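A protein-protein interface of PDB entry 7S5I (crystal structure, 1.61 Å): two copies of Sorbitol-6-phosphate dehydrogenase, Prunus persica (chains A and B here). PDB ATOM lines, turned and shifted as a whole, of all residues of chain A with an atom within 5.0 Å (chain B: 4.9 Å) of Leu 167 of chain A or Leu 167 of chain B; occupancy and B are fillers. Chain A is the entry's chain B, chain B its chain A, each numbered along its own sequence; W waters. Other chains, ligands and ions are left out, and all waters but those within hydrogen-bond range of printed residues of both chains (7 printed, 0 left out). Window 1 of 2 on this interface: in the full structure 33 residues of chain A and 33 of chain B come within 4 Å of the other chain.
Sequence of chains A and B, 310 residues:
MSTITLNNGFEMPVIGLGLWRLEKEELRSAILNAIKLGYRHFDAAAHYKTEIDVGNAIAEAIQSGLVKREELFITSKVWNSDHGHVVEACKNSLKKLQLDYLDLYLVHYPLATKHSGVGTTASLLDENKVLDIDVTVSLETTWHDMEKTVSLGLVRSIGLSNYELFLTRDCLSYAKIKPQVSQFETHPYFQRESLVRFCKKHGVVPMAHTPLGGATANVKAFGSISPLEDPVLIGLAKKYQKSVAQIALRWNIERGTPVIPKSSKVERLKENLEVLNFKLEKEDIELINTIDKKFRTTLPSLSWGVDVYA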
ATOM      1  N   PRO A 110     -14.618  24.365  11.093  1.00  0.00           N
ATOM      2  CA  PRO A 110     -13.218  23.982  11.323  1.00  0.00           C
ATOM      3  C   PRO A 110     -12.694  24.467  12.671  1.00  0.00           C
ATOM      4  O   PRO A 110     -11.650  25.125  12.757  1.00  0.00           O
ATOM      5  CB  PRO A 110     -12.495  24.643  10.149  1.00  0.00           C
ATOM      6  CG  PRO A 110     -13.309  25.931   9.930  1.00  0.00           C
ATOM      7  CD  PRO A 110     -14.745  25.409  10.044  1.00  0.00           C
ATOM      8  N   LEU A 139      -7.936  19.174  13.440  1.00  0.00           N
ATOM      9  CA  LEU A 139      -8.919  18.936  12.397  1.00  0.00           C
ATOM     10  C   LEU A 139      -8.652  17.629  11.665  1.00  0.00           C
ATOM     11  O   LEU A 139      -9.598  16.964  11.218  1.00  0.00           O
ATOM     12  CB  LEU A 139      -8.946  20.119  11.412  1.00  0.00           C
ATOM     13  CG  LEU A 139      -9.401  21.444  12.027  1.00  0.00           C
ATOM     14  CD1 LEU A 139      -9.245  22.563  10.991  1.00  0.00           C
ATOM     15  CD2 LEU A 139     -10.842  21.378  12.508  1.00  0.00           C
ATOM     16  N   ASN A 162     -17.979  25.359   6.200  1.00  0.00           N
ATOM     17  CA  ASN A 162     -17.344  26.618   6.603  1.00  0.00           C
ATOM     18  C   ASN A 162     -15.816  26.530   6.594  1.00  0.00           C
ATOM     19  O   ASN A 162     -15.128  27.252   7.336  1.00  0.00           O
ATOM     20  CB  ASN A 162     -17.854  27.094   7.967  1.00  0.00           C
ATOM     21  CG  ASN A 162     -19.343  27.347   7.964  1.00  0.00           C
ATOM     22  OD1 ASN A 162     -19.874  28.007   7.056  1.00  0.00           O
ATOM     23  ND2 ASN A 162     -20.036  26.815   8.967  1.00  0.00           N
ATOM     24  N   TYR A 163     -15.273  25.658   5.747  1.00  0.00           N
ATOM     25  CA  TYR A 163     -13.837  25.599   5.498  1.00  0.00           C
ATOM     26  C   TYR A 163     -13.538  26.453   4.271  1.00  0.00           C
ATOM     27  O   TYR A 163     -14.315  26.454   3.307  1.00  0.00           O
ATOM     28  CB  TYR A 163     -13.387  24.160   5.225  1.00  0.00           C
ATOM     29  CG  TYR A 163     -13.275  23.217   6.411  1.00  0.00           C
ATOM     30  CD1 TYR A 163     -14.347  23.011   7.273  1.00  0.00           C
ATOM     31  CD2 TYR A 163     -12.101  22.498   6.640  1.00  0.00           C
ATOM     32  CE1 TYR A 163     -14.258  22.129   8.333  1.00  0.00           C
ATOM     33  CE2 TYR A 163     -12.006  21.607   7.707  1.00  0.00           C
ATOM     34  CZ  TYR A 163     -13.088  21.428   8.540  1.00  0.00           C
ATOM     35  OH  TYR A 163     -13.022  20.552   9.604  1.00  0.00           O
ATOM     36  N   GLU A 164     -12.419  27.191   4.299  1.00  0.00           N
ATOM     37  CA  GLU A 164     -12.031  27.993   3.137  1.00  0.00           C
ATOM     38  C   GLU A 164     -10.799  27.366   2.462  1.00  0.00           C
ATOM     39  O   GLU A 164     -10.535  26.177   2.622  1.00  0.00           O
ATOM     40  CB  GLU A 164     -11.835  29.459   3.556  1.00  0.00           C
ATOM     41  CG  GLU A 164     -10.962  29.617   4.791  1.00  0.00           C
ATOM     42  CD  GLU A 164      -9.609  28.960   4.613  1.00  0.00           C
ATOM     43  OE1 GLU A 164      -9.528  27.792   5.005  1.00  0.00           O
ATOM     44  OE2 GLU A 164      -8.655  29.599   4.110  1.00  0.00           O
ATOM     45  N   LEU A 165     -10.060  28.154   1.676  1.00  0.00           N
ATOM     46  CA  LEU A 165      -9.065  27.527   0.802  1.00  0.00           C
ATOM     47  C   LEU A 165      -7.932  26.878   1.597  1.00  0.00           C
ATOM     48  O   LEU A 165      -7.540  25.741   1.313  1.00  0.00           O
ATOM     49  CB  LEU A 165      -8.480  28.546  -0.171  1.00  0.00           C
ATOM     50  CG  LEU A 165      -7.722  27.884  -1.334  1.00  0.00           C
ATOM     51  CD1 LEU A 165      -8.110  28.531  -2.658  1.00  0.00           C
ATOM     52  CD2 LEU A 165      -6.249  27.953  -1.088  1.00  0.00           C
ATOM     53  N   PHE A 166      -7.366  27.589   2.579  1.00  0.00           N
ATOM     54  CA  PHE A 166      -6.226  27.008   3.300  1.00  0.00           C
ATOM     55  C   PHE A 166      -6.627  25.721   4.005  1.00  0.00           C
ATOM     56  O   PHE A 166      -5.877  24.735   4.003  1.00  0.00           O
ATOM     57  CB  PHE A 166      -5.667  27.983   4.339  1.00  0.00           C
ATOM     58  CG  PHE A 166      -5.158  29.293   3.782  1.00  0.00           C
ATOM     59  CD1 PHE A 166      -4.262  29.319   2.724  1.00  0.00           C
ATOM     60  CD2 PHE A 166      -5.536  30.495   4.378  1.00  0.00           C
ATOM     61  CE1 PHE A 166      -3.752  30.530   2.259  1.00  0.00           C
ATOM     62  CE2 PHE A 166      -5.040  31.706   3.918  1.00  0.00           C
ATOM     63  CZ  PHE A 166      -4.136  31.722   2.869  1.00  0.00           C
ATOM     64  N   LEU A 167      -7.801  25.716   4.636  1.00  0.00           N
ATOM     65  CA  LEU A 167      -8.222  24.532   5.386  1.00  0.00           C
ATOM     66  C   LEU A 167      -8.628  23.394   4.458  1.00  0.00           C
ATOM     67  O   LEU A 167      -8.469  22.216   4.810  1.00  0.00           O
ATOM     68  CB  LEU A 167      -9.388  24.890   6.305  1.00  0.00           C
ATOM     69  CG  LEU A 167      -9.079  25.876   7.439  1.00  0.00           C
ATOM     70  CD1 LEU A 167     -10.362  26.556   7.925  1.00  0.00           C
ATOM     71  CD2 LEU A 167      -8.370  25.178   8.592  1.00  0.00           C
ATOM     72  N   THR A 168      -9.190  23.729   3.293  1.00  0.00           N
ATOM     73  CA  THR A 168      -9.605  22.695   2.348  1.00  0.00           C
ATOM     74  C   THR A 168      -8.383  22.044   1.710  1.00  0.00           C
ATOM     75  O   THR A 168      -8.338  20.816   1.582  1.00  0.00           O
ATOM     76  CB  THR A 168     -10.534  23.287   1.290  1.00  0.00           C
ATOM     77  OG1 THR A 168     -11.673  23.872   1.936  1.00  0.00           O
ATOM     78  CG2 THR A 168     -11.026  22.218   0.308  1.00  0.00           C
ATOM     79  N   ARG A 169      -7.391  22.850   1.306  1.00  0.00           N
ATOM     80  CA  ARG A 169      -6.141  22.289   0.799  1.00  0.00           C
ATOM     81  C   ARG A 169      -5.519  21.366   1.832  1.00  0.00           C
ATOM     82  O   ARG A 169      -5.038  20.272   1.503  1.00  0.00           O
ATOM     83  CB  ARG A 169      -5.159  23.397   0.428  1.00  0.00           C
ATOM     84  CG  ARG A 169      -3.891  22.884  -0.289  1.00  0.00           C
ATOM     85  CD  ARG A 169      -2.650  23.731   0.029  1.00  0.00           C
ATOM     86  NE  ARG A 169      -2.201  23.504   1.396  1.00  0.00           N
ATOM     87  CZ  ARG A 169      -1.499  22.453   1.797  1.00  0.00           C
ATOM     88  NH1 ARG A 169      -1.037  21.548   0.934  1.00  0.00           N
ATOM     89  NH2 ARG A 169      -1.302  22.264   3.105  1.00  0.00           N
ATOM     90  N   ASP A 170      -5.544  21.779   3.099  1.00  0.00           N
ATOM     91  CA  ASP A 170      -4.945  20.952   4.143  1.00  0.00           C
ATOM     92  C   ASP A 170      -5.683  19.621   4.259  1.00  0.00           C
ATOM     93  O   ASP A 170      -5.057  18.559   4.314  1.00  0.00           O
ATOM     94  CB  ASP A 170      -4.944  21.714   5.474  1.00  0.00           C
ATOM     95  CG  ASP A 170      -3.815  21.290   6.383  1.00  0.00           C
ATOM     96  OD1 ASP A 170      -2.731  20.949   5.853  1.00  0.00           O
ATOM     97  OD2 ASP A 170      -4.012  21.309   7.625  1.00  0.00           O
ATOM     98  N   CYS A 171      -7.019  19.662   4.273  1.00  0.00           N
ATOM     99  CA  CYS A 171      -7.804  18.428   4.313  1.00  0.00           C
ATOM    100  C   CYS A 171      -7.446  17.507   3.154  1.00  0.00           C
ATOM    101  O   CYS A 171      -7.192  16.310   3.350  1.00  0.00           O
ATOM    102  CB  CYS A 171      -9.297  18.772   4.301  1.00  0.00           C
ATOM    103  SG  CYS A 171     -10.357  17.316   4.346  1.00  0.00           S
ATOM    104  N   PRO B 110       0.110  29.712   5.188  1.00  0.00           N
ATOM    105  CA  PRO B 110      -0.484  28.387   5.432  1.00  0.00           C
ATOM    106  C   PRO B 110      -0.905  27.712   4.132  1.00  0.00           C
ATOM    107  O   PRO B 110      -2.046  27.286   3.976  1.00  0.00           O
ATOM    108  CB  PRO B 110      -1.678  28.716   6.332  1.00  0.00           C
ATOM    109  CG  PRO B 110      -2.118  30.077   5.871  1.00  0.00           C
ATOM    110  CD  PRO B 110      -0.817  30.807   5.550  1.00  0.00           C
ATOM    111  N   LEU B 139      -0.094  21.014   6.510  1.00  0.00           N
ATOM    112  CA  LEU B 139       0.525  22.035   7.347  1.00  0.00           C
ATOM    113  C   LEU B 139       1.163  21.417   8.582  1.00  0.00           C
ATOM    114  O   LEU B 139       2.199  21.906   9.051  1.00  0.00           O
ATOM    115  CB  LEU B 139      -0.496  23.095   7.752  1.00  0.00           C
ATOM    116  CG  LEU B 139      -1.072  23.914   6.587  1.00  0.00           C
ATOM    117  CD1 LEU B 139      -2.112  24.914   7.080  1.00  0.00           C
ATOM    118  CD2 LEU B 139       0.048  24.620   5.817  1.00  0.00           C
ATOM    119  N   ASN B 162       0.728  34.696   8.610  1.00  0.00           N
ATOM    120  CA  ASN B 162      -0.549  34.741   7.872  1.00  0.00           C
ATOM    121  C   ASN B 162      -1.466  33.563   8.199  1.00  0.00           C
ATOM    122  O   ASN B 162      -2.288  33.145   7.365  1.00  0.00           O
ATOM    123  CB  ASN B 162      -0.307  34.849   6.355  1.00  0.00           C
ATOM    124  CG  ASN B 162       0.501  36.063   6.007  1.00  0.00           C
ATOM    125  OD1 ASN B 162       0.188  37.162   6.460  1.00  0.00           O
ATOM    126  ND2 ASN B 162       1.555  35.888   5.213  1.00  0.00           N
ATOM    127  N   TYR B 163      -1.390  33.045   9.425  1.00  0.00           N
ATOM    128  CA  TYR B 163      -2.357  32.064   9.913  1.00  0.00           C
ATOM    129  C   TYR B 163      -3.413  32.796  10.739  1.00  0.00           C
ATOM    130  O   TYR B 163      -3.092  33.743  11.474  1.00  0.00           O
ATOM    131  CB  TYR B 163      -1.686  30.999  10.800  1.00  0.00           C
ATOM    132  CG  TYR B 163      -0.842  29.932  10.131  1.00  0.00           C
ATOM    133  CD1 TYR B 163       0.203  30.276   9.277  1.00  0.00           C
ATOM    134  CD2 TYR B 163      -1.060  28.579  10.411  1.00  0.00           C
ATOM    135  CE1 TYR B 163       1.020  29.298   8.691  1.00  0.00           C
ATOM    136  CE2 TYR B 163      -0.244  27.593   9.840  1.00  0.00           C
ATOM    137  CZ  TYR B 163       0.778  27.961   8.981  1.00  0.00           C
ATOM    138  OH  TYR B 163       1.587  26.995   8.403  1.00  0.00           O
ATOM    139  N   GLU B 164      -4.676  32.391  10.603  1.00  0.00           N
ATOM    140  CA  GLU B 164      -5.738  33.052  11.375  1.00  0.00           C
ATOM    141  C   GLU B 164      -6.230  32.094  12.479  1.00  0.00           C
ATOM    142  O   GLU B 164      -5.513  31.160  12.862  1.00  0.00           O
ATOM    143  CB  GLU B 164      -6.862  33.552  10.453  1.00  0.00           C
ATOM    144  CG  GLU B 164      -7.295  32.541   9.426  1.00  0.00           C
ATOM    145  CD  GLU B 164      -7.766  31.268  10.076  1.00  0.00           C
ATOM    146  OE1 GLU B 164      -6.883  30.399  10.234  1.00  0.00           O
ATOM    147  OE2 GLU B 164      -8.958  31.145  10.422  1.00  0.00           O
ATOM    148  N   LEU B 165      -7.456  32.298  12.976  1.00  0.00           N
ATOM    149  CA  LEU B 165      -7.871  31.579  14.185  1.00  0.00           C
ATOM    150  C   LEU B 165      -7.952  30.072  13.951  1.00  0.00           C
ATOM    151  O   LEU B 165      -7.424  29.281  14.747  1.00  0.00           O
ATOM    152  CB  LEU B 165      -9.218  32.104  14.692  1.00  0.00           C
ATOM    153  CG  LEU B 165      -9.748  31.292  15.888  1.00  0.00           C
ATOM    154  CD1 LEU B 165      -9.034  31.758  17.104  1.00  0.00           C
ATOM    155  CD2 LEU B 165     -11.252  31.517  16.030  1.00  0.00           C
ATOM    156  N   PHE B 166      -8.644  29.649  12.891  1.00  0.00           N
ATOM    157  CA  PHE B 166      -8.817  28.210  12.684  1.00  0.00           C
ATOM    158  C   PHE B 166      -7.475  27.520  12.505  1.00  0.00           C
ATOM    159  O   PHE B 166      -7.219  26.464  13.095  1.00  0.00           O
ATOM    160  CB  PHE B 166      -9.687  27.950  11.451  1.00  0.00           C
ATOM    161  CG  PHE B 166     -11.085  28.538  11.519  1.00  0.00           C
ATOM    162  CD1 PHE B 166     -11.912  28.346  12.638  1.00  0.00           C
ATOM    163  CD2 PHE B 166     -11.586  29.240  10.440  1.00  0.00           C
ATOM    164  CE1 PHE B 166     -13.213  28.879  12.660  1.00  0.00           C
ATOM    165  CE2 PHE B 166     -12.887  29.782  10.452  1.00  0.00           C
ATOM    166  CZ  PHE B 166     -13.698  29.594  11.557  1.00  0.00           C
ATOM    167  N   LEU B 167      -6.595  28.118  11.707  1.00  0.00           N
ATOM    168  CA  LEU B 167      -5.313  27.467  11.441  1.00  0.00           C
ATOM    169  C   LEU B 167      -4.405  27.509  12.661  1.00  0.00           C
ATOM    170  O   LEU B 167      -3.584  26.599  12.857  1.00  0.00           O
ATOM    171  CB  LEU B 167      -4.626  28.159  10.260  1.00  0.00           C
ATOM    172  CG  LEU B 167      -5.383  27.999   8.935  1.00  0.00           C
ATOM    173  CD1 LEU B 167      -4.982  29.141   7.961  1.00  0.00           C
ATOM    174  CD2 LEU B 167      -5.087  26.648   8.343  1.00  0.00           C
ATOM    175  N   THR B 168      -4.504  28.575  13.457  1.00  0.00           N
ATOM    176  CA  THR B 168      -3.659  28.686  14.640  1.00  0.00           C
ATOM    177  C   THR B 168      -4.106  27.711  15.705  1.00  0.00           C
ATOM    178  O   THR B 168      -3.269  27.058  16.336  1.00  0.00           O
ATOM    179  CB  THR B 168      -3.686  30.117  15.177  1.00  0.00           C
ATOM    180  OG1 THR B 168      -3.209  30.988  14.149  1.00  0.00           O
ATOM    181  CG2 THR B 168      -2.786  30.262  16.408  1.00  0.00           C
ATOM    182  N   ARG B 169      -5.424  27.605  15.917  1.00  0.00           N
ATOM    183  CA  ARG B 169      -5.936  26.584  16.838  1.00  0.00           C
ATOM    184  C   ARG B 169      -5.499  25.191  16.406  1.00  0.00           C
ATOM    185  O   ARG B 169      -5.122  24.350  17.234  1.00  0.00           O
ATOM    186  CB  ARG B 169      -7.460  26.642  16.907  1.00  0.00           C
ATOM    187  CG  ARG B 169      -8.026  25.735  18.015  1.00  0.00           C
ATOM    188  CD  ARG B 169      -9.410  25.149  17.654  1.00  0.00           C
ATOM    189  NE  ARG B 169      -9.290  24.139  16.611  1.00  0.00           N
ATOM    190  CZ  ARG B 169      -8.895  22.889  16.798  1.00  0.00           C
ATOM    191  NH1 ARG B 169      -8.713  22.388  18.017  1.00  0.00           N
ATOM    192  NH2 ARG B 169      -8.663  22.121  15.736  1.00  0.00           N
ATOM    193  N   ASP B 170      -5.547  24.923  15.105  1.00  0.00           N
ATOM    194  CA  ASP B 170      -5.116  23.616  14.617  1.00  0.00           C
ATOM    195  C   ASP B 170      -3.644  23.370  14.934  1.00  0.00           C
ATOM    196  O   ASP B 170      -3.281  22.310  15.468  1.00  0.00           O
ATOM    197  CB  ASP B 170      -5.422  23.516  13.127  1.00  0.00           C
ATOM    198  CG  ASP B 170      -5.719  22.113  12.691  1.00  0.00           C
ATOM    199  OD1 ASP B 170      -5.351  21.768  11.549  1.00  0.00           O
ATOM    200  OD2 ASP B 170      -6.215  21.319  13.517  1.00  0.00           O
ATOM    201  N   CYS B 171      -2.786  24.362  14.667  1.00  0.00           N
ATOM    202  CA  CYS B 171      -1.372  24.201  14.984  1.00  0.00           C
ATOM    203  C   CYS B 171      -1.190  23.869  16.472  1.00  0.00           C
ATOM    204  O   CYS B 171      -0.441  22.955  16.826  1.00  0.00           O
ATOM    205  CB  CYS B 171      -0.611  25.473  14.570  1.00  0.00           C
ATOM    206  SG  CYS B 171       1.135  25.427  14.990  1.00  0.00           S
HETATM  207  O   HOH W   1      -5.132  18.963  11.559  1.00  0.00           O
HETATM  208  O   HOH W   2      -9.005  30.598   7.296  1.00  0.00           O
HETATM  209  O   HOH W   3      -2.142  19.678   8.804  1.00  0.00           O
HETATM  210  O   HOH W   4      -9.263  24.704  13.919  1.00  0.00           O
HETATM  211  O   HOH W   5      -3.600  22.895  10.158  1.00  0.00           O
HETATM  212  O   HOH W   6      -6.336  21.378   8.886  1.00  0.00           O
HETATM  213  O   HOH W   7      -3.116  24.852   3.618  1.00  0.00           O
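The backbone NH (N) of Leu 139 of chain B sits at hydrogen-bond distance from the side-chain carboxylate (OD1) of Asp 170 of chain A (2.7 Å).
The side-chain carboxylate of Asp 170 of chain B is in hydrogen-bond range of the backbone NH of Leu 139 of chain A (2.8 Å).
The side-chain carboxylate (OE2) of Glu 164 of chain B lies within hydrogen-bond range of the backbone NH (N) of Phe 166 of chain B, 2.9 Å away.
The backbone NH (N) of Leu 167 of chain B lies within hydrogen-bond range of the side-chain carboxylate (OE1) of Glu 164 of chain B (2.7 Å).
NH2 of Arg 169 of chain B is in salt-bridge range of OD2 of Asp 170 of chain B (3.4 Å).
The backbone NH (N) of Phe 166 of chain A sits at hydrogen-bond distance from the side-chain carboxylate (OE2) of Glu 164 of chain A, 2.8 Å away.
The side-chain carboxylate (OE1) of Glu 164 of chain A is in hydrogen-bond range of the backbone NH (N) of Leu 167 of chain A (2.7 Å).
NH2 of Arg 169 of chain A is in salt-bridge range of OD1 of Asp 170 of chain A, at 3.4 Å.
Pro 110 of chain A touches Phe 166 of chain B.
Arg 169 of chain B touches Leu 139 of chain A.
Pro 110 of chain B touches Phe 166 of chain A.
Phe 166 of chain A touches Leu 167 of chain B (CB to CD1, 3.9 Å).
Phe 166 of chain B touches Leu 167 of chain A (CB to CD1, 3.9 Å).
Leu 167 of chain A touches Leu 167 of chain B.
Arg 169 of chain A touches Leu 139 of chain B (NH2 to N, 3.8 Å).
Of chain B, only Phe 166 (3.9 Å) and Leu 167 (3.6 Å) come within 4 Å of Leu 167 of chain A.
Of the printed residues of chain A, Arg 169 of chain B touches Leu 139 (3.8 Å).
Printed residues of chain B within 4 Å of Phe 166 of chain A: Pro 110 and Leu 167.
Printed residues of chain A within 4 Å of Asp 170 of chain B: Leu 139 (2.8 Å).
Tyr 163 of chain B touches none of the printed residues of chain A.
Thr 168 of chain A touches none of the printed residues of chain B.
The nearest printed residue of chain B that does not touch Leu 167 of chain A is Glu 164 of chain B (5.4 Å).
The nearest printed residue of chain A that does not touch Leu 167 of chain B is Glu 164 of chain A (5.3 Å).
Hydrophobic or aromatic side chains of chain A within 4 Å of the printed part of chain B: Pro 110, Leu 139, Phe 166 and Leu 167.
Pro 110 of chain A touches Phe 166 of chain B, and with the chains exchanged Phe 166 of chain A touches Pro 110 of chain B.
Leu 139 of chain A touches Arg 169 of chain B, and with the chains exchanged Arg 169 of chain A touches Leu 139 of chain B.
Phe 166 of chain A touches Leu 167 of chain B, and with the chains exchanged Leu 167 of chain A touches Phe 166 of chain B.
Leu 167 of chain B touches its own counterpart, Leu 167 of chain A.
12 positions are printed for both chains.
Water W5 lies within hydrogen-bond range of OD1 of Asp 170 of chain B (2.5 Å) and OD2 of Asp 170 of chain A (3.0 Å).
Water W6 lies within hydrogen-bond range of the side-chain carboxylate (OD2) of Asp 170 of chain A and the side-chain carboxylate (OD1) of Asp 170 of chain B.
Water W7 lies within hydrogen-bond range of O of Pro 110 of chain B, NE of Arg 169 of chain A and O of Phe 166 of chain A.
Water W4 lies within hydrogen-bond range of the backbone carbonyl oxygen (O) of Pro 110 of chain A, the guanidinium group (NE) of Arg 169 of chain B and the backbone carbonyl oxygen (O) of Phe 166 of chain B.
Water W1 lies within hydrogen-bond range of OD1 of Asp 170 of chain B and N of Leu 139 of chain A.
Water W2 bridges OE2 of Glu 164 of chain B (3.2 Å) and OE2 of Glu 164 of chain A (3.4 Å).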
